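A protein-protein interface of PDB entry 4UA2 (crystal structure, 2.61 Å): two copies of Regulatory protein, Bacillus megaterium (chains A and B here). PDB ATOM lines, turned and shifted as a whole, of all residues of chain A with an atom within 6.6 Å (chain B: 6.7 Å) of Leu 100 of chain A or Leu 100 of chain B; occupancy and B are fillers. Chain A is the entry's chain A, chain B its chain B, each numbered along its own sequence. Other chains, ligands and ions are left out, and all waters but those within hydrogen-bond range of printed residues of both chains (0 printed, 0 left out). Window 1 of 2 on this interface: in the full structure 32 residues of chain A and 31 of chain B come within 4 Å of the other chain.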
ATOM      1  N   LEU A  58     -11.056  -5.740  20.857  1.00  0.00           N
ATOM      2  CA  LEU A  58      -9.784  -5.085  20.573  1.00  0.00           C
ATOM      3  C   LEU A  58      -8.759  -5.267  21.695  1.00  0.00           C
ATOM      4  O   LEU A  58      -7.682  -4.671  21.662  1.00  0.00           O
ATOM      5  CB  LEU A  58     -10.011  -3.602  20.285  1.00  0.00           C
ATOM      6  CG  LEU A  58     -10.706  -3.386  18.937  1.00  0.00           C
ATOM      7  CD1 LEU A  58     -10.854  -1.914  18.613  1.00  0.00           C
ATOM      8  CD2 LEU A  58      -9.951  -4.104  17.826  1.00  0.00           C
ATOM      9  N   GLY A  59      -9.103  -6.083  22.687  1.00  0.00           N
ATOM     10  CA  GLY A  59      -8.154  -6.465  23.717  1.00  0.00           C
ATOM     11  C   GLY A  59      -8.359  -5.831  25.080  1.00  0.00           C
ATOM     12  O   GLY A  59      -7.576  -6.065  26.000  1.00  0.00           O
ATOM     13  N   PHE A  60      -9.409  -5.029  25.215  1.00  0.00           N
ATOM     14  CA  PHE A  60      -9.715  -4.391  26.490  1.00  0.00           C
ATOM     15  C   PHE A  60     -10.491  -5.324  27.418  1.00  0.00           C
ATOM     16  O   PHE A  60     -11.381  -6.054  26.979  1.00  0.00           O
ATOM     17  CB  PHE A  60     -10.504  -3.101  26.268  1.00  0.00           C
ATOM     18  CG  PHE A  60      -9.672  -1.961  25.755  1.00  0.00           C
ATOM     19  CD1 PHE A  60      -9.138  -1.029  26.632  1.00  0.00           C
ATOM     20  CD2 PHE A  60      -9.425  -1.816  24.400  1.00  0.00           C
ATOM     21  CE1 PHE A  60      -8.373   0.024  26.167  1.00  0.00           C
ATOM     22  CE2 PHE A  60      -8.661  -0.764  23.928  1.00  0.00           C
ATOM     23  CZ  PHE A  60      -8.134   0.156  24.813  1.00  0.00           C
ATOM     24  N   ILE A  93      -1.751   0.587  23.241  1.00  0.00           N
ATOM     25  CA  ILE A  93      -2.449   0.673  21.969  1.00  0.00           C
ATOM     26  C   ILE A  93      -1.551   1.257  20.880  1.00  0.00           C
ATOM     27  O   ILE A  93      -1.720   0.943  19.704  1.00  0.00           O
ATOM     28  CB  ILE A  93      -3.747   1.507  22.102  1.00  0.00           C
ATOM     29  CG1 ILE A  93      -4.719   1.182  20.969  1.00  0.00           C
ATOM     30  CG2 ILE A  93      -3.450   3.000  22.161  1.00  0.00           C
ATOM     31  CD1 ILE A  93      -6.089   1.777  21.176  1.00  0.00           C
ATOM     32  N   ARG A  95       1.844   0.768  20.687  1.00  0.00           N
ATOM     33  CA  ARG A  95       2.694  -0.347  20.276  1.00  0.00           C
ATOM     34  C   ARG A  95       1.913  -1.331  19.403  1.00  0.00           C
ATOM     35  O   ARG A  95       2.405  -1.792  18.361  1.00  0.00           O
ATOM     36  CB  ARG A  95       3.278  -1.060  21.497  1.00  0.00           C
ATOM     37  CG  ARG A  95       4.012  -0.135  22.455  1.00  0.00           C
ATOM     38  CD  ARG A  95       5.039   0.720  21.729  1.00  0.00           C
ATOM     39  NE  ARG A  95       5.644   1.715  22.611  1.00  0.00           N
ATOM     40  N   LYS A  96       0.687  -1.633  19.826  1.00  0.00           N
ATOM     41  CA  LYS A  96      -0.194  -2.522  19.073  1.00  0.00           C
ATOM     42  C   LYS A  96      -0.429  -2.006  17.652  1.00  0.00           C
ATOM     43  O   LYS A  96      -0.332  -2.762  16.681  1.00  0.00           O
ATOM     44  CB  LYS A  96      -1.526  -2.690  19.809  1.00  0.00           C
ATOM     45  CG  LYS A  96      -2.501  -3.654  19.154  1.00  0.00           C
ATOM     46  CD  LYS A  96      -3.771  -3.784  19.985  1.00  0.00           C
ATOM     47  CE  LYS A  96      -4.842  -4.592  19.267  1.00  0.00           C
ATOM     48  NZ  LYS A  96      -4.420  -5.993  19.003  1.00  0.00           N
ATOM     49  N   ILE A  97      -0.726  -0.713  17.541  1.00  0.00           N
ATOM     50  CA  ILE A  97      -0.949  -0.074  16.246  1.00  0.00           C
ATOM     51  C   ILE A  97       0.280  -0.185  15.347  1.00  0.00           C
ATOM     52  O   ILE A  97       0.163  -0.541  14.172  1.00  0.00           O
ATOM     53  CB  ILE A  97      -1.329   1.414  16.408  1.00  0.00           C
ATOM     54  CG1 ILE A  97      -2.778   1.545  16.873  1.00  0.00           C
ATOM     55  CG2 ILE A  97      -1.152   2.163  15.096  1.00  0.00           C
ATOM     56  CD1 ILE A  97      -3.153   2.944  17.305  1.00  0.00           C
ATOM     57  N   GLU A  98       1.452   0.116  15.900  1.00  0.00           N
ATOM     58  CA  GLU A  98       2.700   0.008  15.143  1.00  0.00           C
ATOM     59  C   GLU A  98       2.905  -1.404  14.597  1.00  0.00           C
ATOM     60  O   GLU A  98       3.166  -1.595  13.396  1.00  0.00           O
ATOM     61  CB  GLU A  98       3.889   0.408  16.016  1.00  0.00           C
ATOM     62  CG  GLU A  98       3.856   1.852  16.484  1.00  0.00           C
ATOM     63  CD  GLU A  98       4.918   2.147  17.522  1.00  0.00           C
ATOM     64  OE1 GLU A  98       5.626   1.202  17.933  1.00  0.00           O
ATOM     65  OE2 GLU A  98       5.047   3.320  17.928  1.00  0.00           O
ATOM     66  N   ASP A  99       2.778  -2.389  15.485  1.00  0.00           N
ATOM     67  CA  ASP A  99       2.906  -3.787  15.092  1.00  0.00           C
ATOM     68  C   ASP A  99       1.950  -4.137  13.957  1.00  0.00           C
ATOM     69  O   ASP A  99       2.366  -4.681  12.931  1.00  0.00           O
ATOM     70  CB  ASP A  99       2.657  -4.711  16.286  1.00  0.00           C
ATOM     71  CG  ASP A  99       3.791  -4.686  17.290  1.00  0.00           C
ATOM     72  OD1 ASP A  99       4.863  -4.133  16.966  1.00  0.00           O
ATOM     73  OD2 ASP A  99       3.614  -5.227  18.402  1.00  0.00           O
ATOM     74  N   LEU A 100       0.674  -3.804  14.134  1.00  0.00           N
ATOM     75  CA  LEU A 100      -0.339  -4.109  13.127  1.00  0.00           C
ATOM     76  C   LEU A 100      -0.058  -3.423  11.789  1.00  0.00           C
ATOM     77  O   LEU A 100      -0.342  -3.982  10.731  1.00  0.00           O
ATOM     78  CB  LEU A 100      -1.730  -3.717  13.631  1.00  0.00           C
ATOM     79  CG  LEU A 100      -2.300  -4.575  14.762  1.00  0.00           C
ATOM     80  CD1 LEU A 100      -3.728  -4.167  15.070  1.00  0.00           C
ATOM     81  CD2 LEU A 100      -2.228  -6.053  14.411  1.00  0.00           C
ATOM     82  N   LYS A 101       0.497  -2.215  11.835  1.00  0.00           N
ATOM     83  CA  LYS A 101       0.842  -1.501  10.609  1.00  0.00           C
ATOM     84  C   LYS A 101       1.961  -2.213   9.857  1.00  0.00           C
ATOM     85  O   LYS A 101       1.871  -2.419   8.639  1.00  0.00           O
ATOM     86  CB  LYS A 101       1.246  -0.057  10.912  1.00  0.00           C
ATOM     87  CG  LYS A 101       0.077   0.916  10.944  1.00  0.00           C
ATOM     88  CD  LYS A 101       0.558   2.351  11.082  1.00  0.00           C
ATOM     89  CE  LYS A 101      -0.586   3.334  10.907  1.00  0.00           C
ATOM     90  NZ  LYS A 101      -1.202   3.236   9.553  1.00  0.00           N
ATOM     91  N   ARG A 102       3.014  -2.589  10.581  1.00  0.00           N
ATOM     92  CA  ARG A 102       4.106  -3.333   9.958  1.00  0.00           C
ATOM     93  C   ARG A 102       3.608  -4.650   9.364  1.00  0.00           C
ATOM     94  O   ARG A 102       3.973  -5.015   8.242  1.00  0.00           O
ATOM     95  CB  ARG A 102       5.229  -3.601  10.960  1.00  0.00           C
ATOM     96  CG  ARG A 102       6.079  -2.384  11.279  1.00  0.00           C
ATOM     97  CD  ARG A 102       7.368  -2.782  11.977  1.00  0.00           C
ATOM     98  NE  ARG A 102       7.116  -3.587  13.167  1.00  0.00           N
ATOM     99  CZ  ARG A 102       6.864  -3.083  14.370  1.00  0.00           C
ATOM    100  NH1 ARG A 102       6.829  -1.770  14.545  1.00  0.00           N
ATOM    101  NH2 ARG A 102       6.647  -3.891  15.399  1.00  0.00           N
ATOM    102  N   ILE A 103       2.765  -5.352  10.117  1.00  0.00           N
ATOM    103  CA  ILE A 103       2.193  -6.614   9.656  1.00  0.00           C
ATOM    104  C   ILE A 103       1.360  -6.409   8.395  1.00  0.00           C
ATOM    105  O   ILE A 103       1.382  -7.236   7.483  1.00  0.00           O
ATOM    106  CB  ILE A 103       1.323  -7.269  10.748  1.00  0.00           C
ATOM    107  CG1 ILE A 103       2.185  -7.655  11.948  1.00  0.00           C
ATOM    108  CG2 ILE A 103       0.614  -8.504  10.212  1.00  0.00           C
ATOM    109  CD1 ILE A 103       1.393  -8.214  13.097  1.00  0.00           C
ATOM    110  N   GLU A 104       0.639  -5.293   8.341  1.00  0.00           N
ATOM    111  CA  GLU A 104      -0.184  -4.978   7.180  1.00  0.00           C
ATOM    112  C   GLU A 104       0.682  -4.725   5.949  1.00  0.00           C
ATOM    113  O   GLU A 104       0.383  -5.219   4.860  1.00  0.00           O
ATOM    114  CB  GLU A 104      -1.073  -3.765   7.455  1.00  0.00           C
ATOM    115  CG  GLU A 104      -2.100  -3.505   6.365  1.00  0.00           C
ATOM    116  CD  GLU A 104      -2.934  -2.268   6.628  1.00  0.00           C
ATOM    117  OE1 GLU A 104      -2.395  -1.293   7.192  1.00  0.00           O
ATOM    118  OE2 GLU A 104      -4.131  -2.273   6.273  1.00  0.00           O
ATOM    119  N   ARG A 105       1.755  -3.955   6.123  1.00  0.00           N
ATOM    120  CA  ARG A 105       2.677  -3.704   5.018  1.00  0.00           C
ATOM    121  C   ARG A 105       3.326  -5.005   4.547  1.00  0.00           C
ATOM    122  O   ARG A 105       3.590  -5.185   3.355  1.00  0.00           O
ATOM    123  CB  ARG A 105       3.751  -2.690   5.421  1.00  0.00           C
ATOM    124  CG  ARG A 105       3.279  -1.245   5.374  1.00  0.00           C
ATOM    125  CD  ARG A 105       4.438  -0.270   5.511  1.00  0.00           C
ATOM    126  NE  ARG A 105       5.072  -0.346   6.823  1.00  0.00           N
ATOM    127  CZ  ARG A 105       4.675   0.348   7.885  1.00  0.00           C
ATOM    128  NH1 ARG A 105       3.641   1.172   7.792  1.00  0.00           N
ATOM    129  NH2 ARG A 105       5.311   0.217   9.041  1.00  0.00           N
ATOM    130  N   LEU A 107       1.846  -7.993   4.726  1.00  0.00           N
ATOM    131  CA  LEU A 107       0.781  -8.702   4.019  1.00  0.00           C
ATOM    132  C   LEU A 107       0.590  -8.165   2.604  1.00  0.00           C
ATOM    133  O   LEU A 107       0.382  -8.930   1.663  1.00  0.00           O
ATOM    134  CB  LEU A 107      -0.533  -8.601   4.797  1.00  0.00           C
ATOM    135  CG  LEU A 107      -0.682  -9.498   6.026  1.00  0.00           C
ATOM    136  CD1 LEU A 107      -1.845  -9.032   6.887  1.00  0.00           C
ATOM    137  CD2 LEU A 107      -0.881 -10.944   5.603  1.00  0.00           C
ATOM    138  N   LEU B  58      -1.480 -10.674  18.875  1.00  0.00           N
ATOM    139  CA  LEU B  58      -2.178  -9.651  18.102  1.00  0.00           C
ATOM    140  C   LEU B  58      -3.465 -10.163  17.452  1.00  0.00           C
ATOM    141  O   LEU B  58      -4.108  -9.444  16.688  1.00  0.00           O
ATOM    142  CB  LEU B  58      -1.242  -9.069  17.043  1.00  0.00           C
ATOM    143  CG  LEU B  58      -0.133  -8.196  17.637  1.00  0.00           C
ATOM    144  CD1 LEU B  58       0.941  -7.896  16.612  1.00  0.00           C
ATOM    145  CD2 LEU B  58      -0.712  -6.907  18.200  1.00  0.00           C
ATOM    146  N   GLY B  59      -3.834 -11.405  17.755  1.00  0.00           N
ATOM    147  CA  GLY B  59      -5.113 -11.939  17.320  1.00  0.00           C
ATOM    148  C   GLY B  59      -5.083 -12.960  16.198  1.00  0.00           C
ATOM    149  O   GLY B  59      -6.134 -13.403  15.736  1.00  0.00           O
ATOM    150  N   PHE B  60      -3.888 -13.338  15.756  1.00  0.00           N
ATOM    151  CA  PHE B  60      -3.757 -14.330  14.691  1.00  0.00           C
ATOM    152  C   PHE B  60      -3.796 -15.758  15.233  1.00  0.00           C
ATOM    153  O   PHE B  60      -3.157 -16.071  16.239  1.00  0.00           O
ATOM    154  CB  PHE B  60      -2.463 -14.103  13.909  1.00  0.00           C
ATOM    155  CG  PHE B  60      -2.442 -12.820  13.128  1.00  0.00           C
ATOM    156  CD1 PHE B  60      -2.025 -11.639  13.720  1.00  0.00           C
ATOM    157  CD2 PHE B  60      -2.835 -12.796  11.800  1.00  0.00           C
ATOM    158  CE1 PHE B  60      -2.001 -10.458  13.001  1.00  0.00           C
ATOM    159  CE2 PHE B  60      -2.815 -11.617  11.076  1.00  0.00           C
ATOM    160  CZ  PHE B  60      -2.397 -10.447  11.678  1.00  0.00           C
ATOM    161  N   ILE B  93      -7.249  -6.329   9.405  1.00  0.00           N
ATOM    162  CA  ILE B  93      -6.241  -5.607  10.168  1.00  0.00           C
ATOM    163  C   ILE B  93      -6.341  -4.100   9.926  1.00  0.00           C
ATOM    164  O   ILE B  93      -5.998  -3.309  10.801  1.00  0.00           O
ATOM    165  CB  ILE B  93      -4.812  -6.112   9.833  1.00  0.00           C
ATOM    166  CG1 ILE B  93      -3.842  -5.791  10.969  1.00  0.00           C
ATOM    167  CG2 ILE B  93      -4.312  -5.546   8.511  1.00  0.00           C
ATOM    168  CD1 ILE B  93      -2.470  -6.390  10.768  1.00  0.00           C
ATOM    169  N   ARG B  95      -9.260  -2.490   9.390  1.00  0.00           N
ATOM    170  CA  ARG B  95     -10.374  -2.120  10.259  1.00  0.00           C
ATOM    171  C   ARG B  95      -9.894  -1.967  11.702  1.00  0.00           C
ATOM    172  O   ARG B  95     -10.184  -0.958  12.373  1.00  0.00           O
ATOM    173  CB  ARG B  95     -11.493  -3.159  10.177  1.00  0.00           C
ATOM    174  N   LYS B  96      -9.146  -2.968  12.164  1.00  0.00           N
ATOM    175  CA  LYS B  96      -8.573  -2.934  13.508  1.00  0.00           C
ATOM    176  C   LYS B  96      -7.726  -1.682  13.737  1.00  0.00           C
ATOM    177  O   LYS B  96      -7.870  -1.014  14.759  1.00  0.00           O
ATOM    178  CB  LYS B  96      -7.728  -4.183  13.769  1.00  0.00           C
ATOM    179  CG  LYS B  96      -8.534  -5.417  14.136  1.00  0.00           C
ATOM    180  CD  LYS B  96      -7.623  -6.568  14.528  1.00  0.00           C
ATOM    181  CE  LYS B  96      -8.422  -7.806  14.902  1.00  0.00           C
ATOM    182  NZ  LYS B  96      -7.536  -8.940  15.288  1.00  0.00           N
ATOM    183  N   ILE B  97      -6.854  -1.368  12.783  1.00  0.00           N
ATOM    184  CA  ILE B  97      -5.975  -0.205  12.894  1.00  0.00           C
ATOM    185  C   ILE B  97      -6.768   1.098  13.000  1.00  0.00           C
ATOM    186  O   ILE B  97      -6.468   1.944  13.846  1.00  0.00           O
ATOM    187  CB  ILE B  97      -5.002  -0.118  11.699  1.00  0.00           C
ATOM    188  CG1 ILE B  97      -3.929  -1.202  11.810  1.00  0.00           C
ATOM    189  CG2 ILE B  97      -4.340   1.250  11.639  1.00  0.00           C
ATOM    190  CD1 ILE B  97      -2.996  -1.262  10.621  1.00  0.00           C
ATOM    191  N   GLU B  98      -7.779   1.257  12.149  1.00  0.00           N
ATOM    192  CA  GLU B  98      -8.636   2.442  12.211  1.00  0.00           C
ATOM    193  C   GLU B  98      -9.271   2.592  13.600  1.00  0.00           C
ATOM    194  O   GLU B  98      -9.158   3.652  14.259  1.00  0.00           O
ATOM    195  CB  GLU B  98      -9.724   2.371  11.135  1.00  0.00           C
ATOM    196  CG  GLU B  98      -9.194   2.396   9.708  1.00  0.00           C
ATOM    197  CD  GLU B  98     -10.244   1.995   8.687  1.00  0.00           C
ATOM    198  OE1 GLU B  98      -9.956   2.068   7.474  1.00  0.00           O
ATOM    199  OE2 GLU B  98     -11.356   1.604   9.099  1.00  0.00           O
ATOM    200  N   ASP B  99      -9.926   1.518  14.042  1.00  0.00           N
ATOM    201  CA  ASP B  99     -10.576   1.510  15.352  1.00  0.00           C
ATOM    202  C   ASP B  99      -9.604   1.894  16.469  1.00  0.00           C
ATOM    203  O   ASP B  99      -9.892   2.779  17.279  1.00  0.00           O
ATOM    204  CB  ASP B  99     -11.189   0.137  15.636  1.00  0.00           C
ATOM    205  CG  ASP B  99     -12.410  -0.146  14.779  1.00  0.00           C
ATOM    206  OD1 ASP B  99     -12.993   0.815  14.233  1.00  0.00           O
ATOM    207  OD2 ASP B  99     -12.790  -1.330  14.657  1.00  0.00           O
ATOM    208  N   LEU B 100      -8.448   1.239  16.488  1.00  0.00           N
ATOM    209  CA  LEU B 100      -7.435   1.484  17.510  1.00  0.00           C
ATOM    210  C   LEU B 100      -6.913   2.915  17.494  1.00  0.00           C
ATOM    211  O   LEU B 100      -6.659   3.497  18.548  1.00  0.00           O
ATOM    212  CB  LEU B 100      -6.264   0.520  17.338  1.00  0.00           C
ATOM    213  CG  LEU B 100      -6.530  -0.955  17.624  1.00  0.00           C
ATOM    214  CD1 LEU B 100      -5.332  -1.772  17.196  1.00  0.00           C
ATOM    215  CD2 LEU B 100      -6.840  -1.181  19.093  1.00  0.00           C
ATOM    216  N   LYS B 101      -6.735   3.475  16.301  1.00  0.00           N
ATOM    217  CA  LYS B 101      -6.288   4.857  16.196  1.00  0.00           C
ATOM    218  C   LYS B 101      -7.289   5.779  16.870  1.00  0.00           C
ATOM    219  O   LYS B 101      -6.903   6.686  17.624  1.00  0.00           O
ATOM    220  CB  LYS B 101      -6.093   5.268  14.738  1.00  0.00           C
ATOM    221  CG  LYS B 101      -4.723   4.941  14.194  1.00  0.00           C
ATOM    222  CD  LYS B 101      -4.482   5.627  12.870  1.00  0.00           C
ATOM    223  CE  LYS B 101      -3.025   5.515  12.477  1.00  0.00           C
ATOM    224  NZ  LYS B 101      -2.135   6.173  13.478  1.00  0.00           N
ATOM    225  N   ARG B 102      -8.574   5.529  16.603  1.00  0.00           N
ATOM    226  CA  ARG B 102      -9.644   6.365  17.149  1.00  0.00           C
ATOM    227  C   ARG B 102      -9.729   6.226  18.662  1.00  0.00           C
ATOM    228  O   ARG B 102      -9.899   7.216  19.376  1.00  0.00           O
ATOM    229  CB  ARG B 102     -10.982   6.017  16.500  1.00  0.00           C
ATOM    230  CG  ARG B 102     -11.487   7.089  15.565  1.00  0.00           C
ATOM    231  CD  ARG B 102     -12.678   6.610  14.825  1.00  0.00           C
ATOM    232  NE  ARG B 102     -12.320   5.511  13.909  1.00  0.00           N
ATOM    233  CZ  ARG B 102     -12.570   4.232  14.160  1.00  0.00           C
ATOM    234  NH1 ARG B 102     -13.183   3.879  15.293  1.00  0.00           N
ATOM    235  NH2 ARG B 102     -12.219   3.324  13.277  1.00  0.00           N
ATOM    236  N   ILE B 103      -9.570   5.000  19.149  1.00  0.00           N
ATOM    237  CA  ILE B 103      -9.570   4.753  20.582  1.00  0.00           C
ATOM    238  C   ILE B 103      -8.414   5.498  21.232  1.00  0.00           C
ATOM    239  O   ILE B 103      -8.560   6.079  22.308  1.00  0.00           O
ATOM    240  CB  ILE B 103      -9.473   3.252  20.888  1.00  0.00           C
ATOM    241  CG1 ILE B 103     -10.697   2.530  20.330  1.00  0.00           C
ATOM    242  CG2 ILE B 103      -9.357   3.008  22.382  1.00  0.00           C
ATOM    243  CD1 ILE B 103     -10.639   1.046  20.502  1.00  0.00           C
ATOM    244  N   GLU B 104      -7.273   5.503  20.553  1.00  0.00           N
ATOM    245  CA  GLU B 104      -6.097   6.197  21.055  1.00  0.00           C
ATOM    246  C   GLU B 104      -6.355   7.696  21.160  1.00  0.00           C
ATOM    247  O   GLU B 104      -6.005   8.318  22.165  1.00  0.00           O
ATOM    248  CB  GLU B 104      -4.885   5.933  20.164  1.00  0.00           C
ATOM    249  CG  GLU B 104      -3.588   6.480  20.740  1.00  0.00           C
ATOM    250  CD  GLU B 104      -2.396   6.246  19.836  1.00  0.00           C
ATOM    251  OE1 GLU B 104      -2.604   5.940  18.644  1.00  0.00           O
ATOM    252  OE2 GLU B 104      -1.250   6.367  20.318  1.00  0.00           O
ATOM    253  N   ARG B 105      -6.967   8.272  20.129  1.00  0.00           N
ATOM    254  CA  ARG B 105      -7.314   9.692  20.176  1.00  0.00           C
ATOM    255  C   ARG B 105      -8.322   9.984  21.289  1.00  0.00           C
ATOM    256  O   ARG B 105      -8.284  11.051  21.908  1.00  0.00           O
ATOM    257  CB  ARG B 105      -7.860  10.165  18.827  1.00  0.00           C
ATOM    258  CG  ARG B 105      -6.780  10.404  17.783  1.00  0.00           C
ATOM    259  CD  ARG B 105      -7.324  11.149  16.575  1.00  0.00           C
ATOM    260  NE  ARG B 105      -8.321  10.370  15.849  1.00  0.00           N
ATOM    261  CZ  ARG B 105      -8.033   9.513  14.876  1.00  0.00           C
ATOM    262  NH1 ARG B 105      -6.773   9.322  14.511  1.00  0.00           N
ATOM    263  NH2 ARG B 105      -9.002   8.845  14.267  1.00  0.00           N
ATOM    264  N   LEU B 107      -8.539   8.269  24.194  1.00  0.00           N
ATOM    265  CA  LEU B 107      -7.751   8.197  25.417  1.00  0.00           C
ATOM    266  C   LEU B 107      -6.905   9.449  25.604  1.00  0.00           C
ATOM    267  O   LEU B 107      -6.682   9.896  26.729  1.00  0.00           O
ATOM    268  CB  LEU B 107      -6.859   6.955  25.403  1.00  0.00           C
ATOM    269  CG  LEU B 107      -7.584   5.611  25.475  1.00  0.00           C
ATOM    270  CD1 LEU B 107      -6.640   4.474  25.127  1.00  0.00           C
ATOM    271  CD2 LEU B 107      -8.185   5.408  26.858  1.00  0.00           C
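The side-chain carboxylate (OD1) of Asp 99 of chain A is in salt-bridge range of the guanidinium group (NH1) of Arg 102 of chain A (3.9 Å).
NH2 of Arg 102 of chain B is in salt-bridge range of OD1 of Asp 99 of chain B (2.8 Å).
Ile 93 of chain A touches Ile 103 of chain B (CD1 to CG2, 3.7 Å).
CG of Lys 96 of chain A touches CD2 of Leu 58 of chain B (3.8 Å).
Ile 97 of chain A touches Lys 101 of chain B.
Glu 104 of chain B touches Ile 97 of chain A.
Leu 58 of chain B touches Asp 99 of chain A.
Leu 100 of chain A touches Ile 97 of chain B (O to CD1, 3.8 Å).
CD1 of Leu 100 of chain A touches CD1 of Leu 100 of chain B (3.6 Å).
Ile 103 of chain A touches Phe 60 of chain B.
Ile 93 of chain B touches Ile 103 of chain A (CD1 to CG2, 3.8 Å).
CD1 of Ile 97 of chain B touches OE1 of Glu 104 of chain A, 3.5 Å away.
Leu 100 of chain A touches just these residues of chain B: Ile 93, Ile 97 and Leu 100.
Of chain A, only Ile 93 (3.2 Å), Lys 96 (3.5 Å), Ile 97 (3.7 Å) and Leu 100 (3.6 Å) come within 4 Å of Leu 100 of chain B.
Of the printed residues of chain B, Ile 93 of chain A touches Leu 100 (3.2 Å), Ile 103 (3.7 Å) and Glu 104 (3.8 Å).
Of the printed residues of chain B, Glu 104 of chain A touches Ile 93 (3.7 Å) and Ile 97 (3.5 Å).
Of the printed residues of chain B, Lys 101 of chain A touches Ile 97 (3.8 Å) and Lys 101 (3.6 Å).
Of the printed residues of chain B, Leu 58 of chain A touches Asp 99 and Ile 103.
Lys 96 of chain B touches none of the printed residues of chain A.
Arg 95 of chain B touches none of the printed residues of chain A.
The nearest residue of chain B that does not touch Leu 100 of chain A is Leu 58 of chain B (4.1 Å).
The nearest printed residue of chain B that does not touch Ile 93 of chain A is Leu 107 of chain B (4.6 Å).
Hydrophobic or aromatic side chains of chain A within 4 Å of the printed part of chain B: Leu 58, Phe 60, Ile 93, Ile 97, Leu 100 and Ile 103.
Among the printed residues, no Asp or Glu carboxylate lies within 4 Å of a Lys or Arg side-chain nitrogen of the other chain.
Lys 96 of chain A touches Leu 58 of chain B, but with the chains exchanged Leu 58 of chain A does not touch Lys 96 of chain B (4.2 Å).
Lys 96 of chain A touches Leu 100 of chain B, but with the chains exchanged Leu 100 of chain A does not touch Lys 96 of chain B (4.2 Å).
Ile 97 of chain A touches Leu 100 of chain B, and with the chains exchanged Leu 100 of chain A touches Ile 97 of chain B.
Ile 97 of chain A touches Lys 101 of chain B, and with the chains exchanged Lys 101 of chain A touches Ile 97 of chain B.
16 positions are printed for both chains.
Of the 22 pairs that touch across the chains among the printed residues, 20 have their exchanged pair printed and touching as well.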
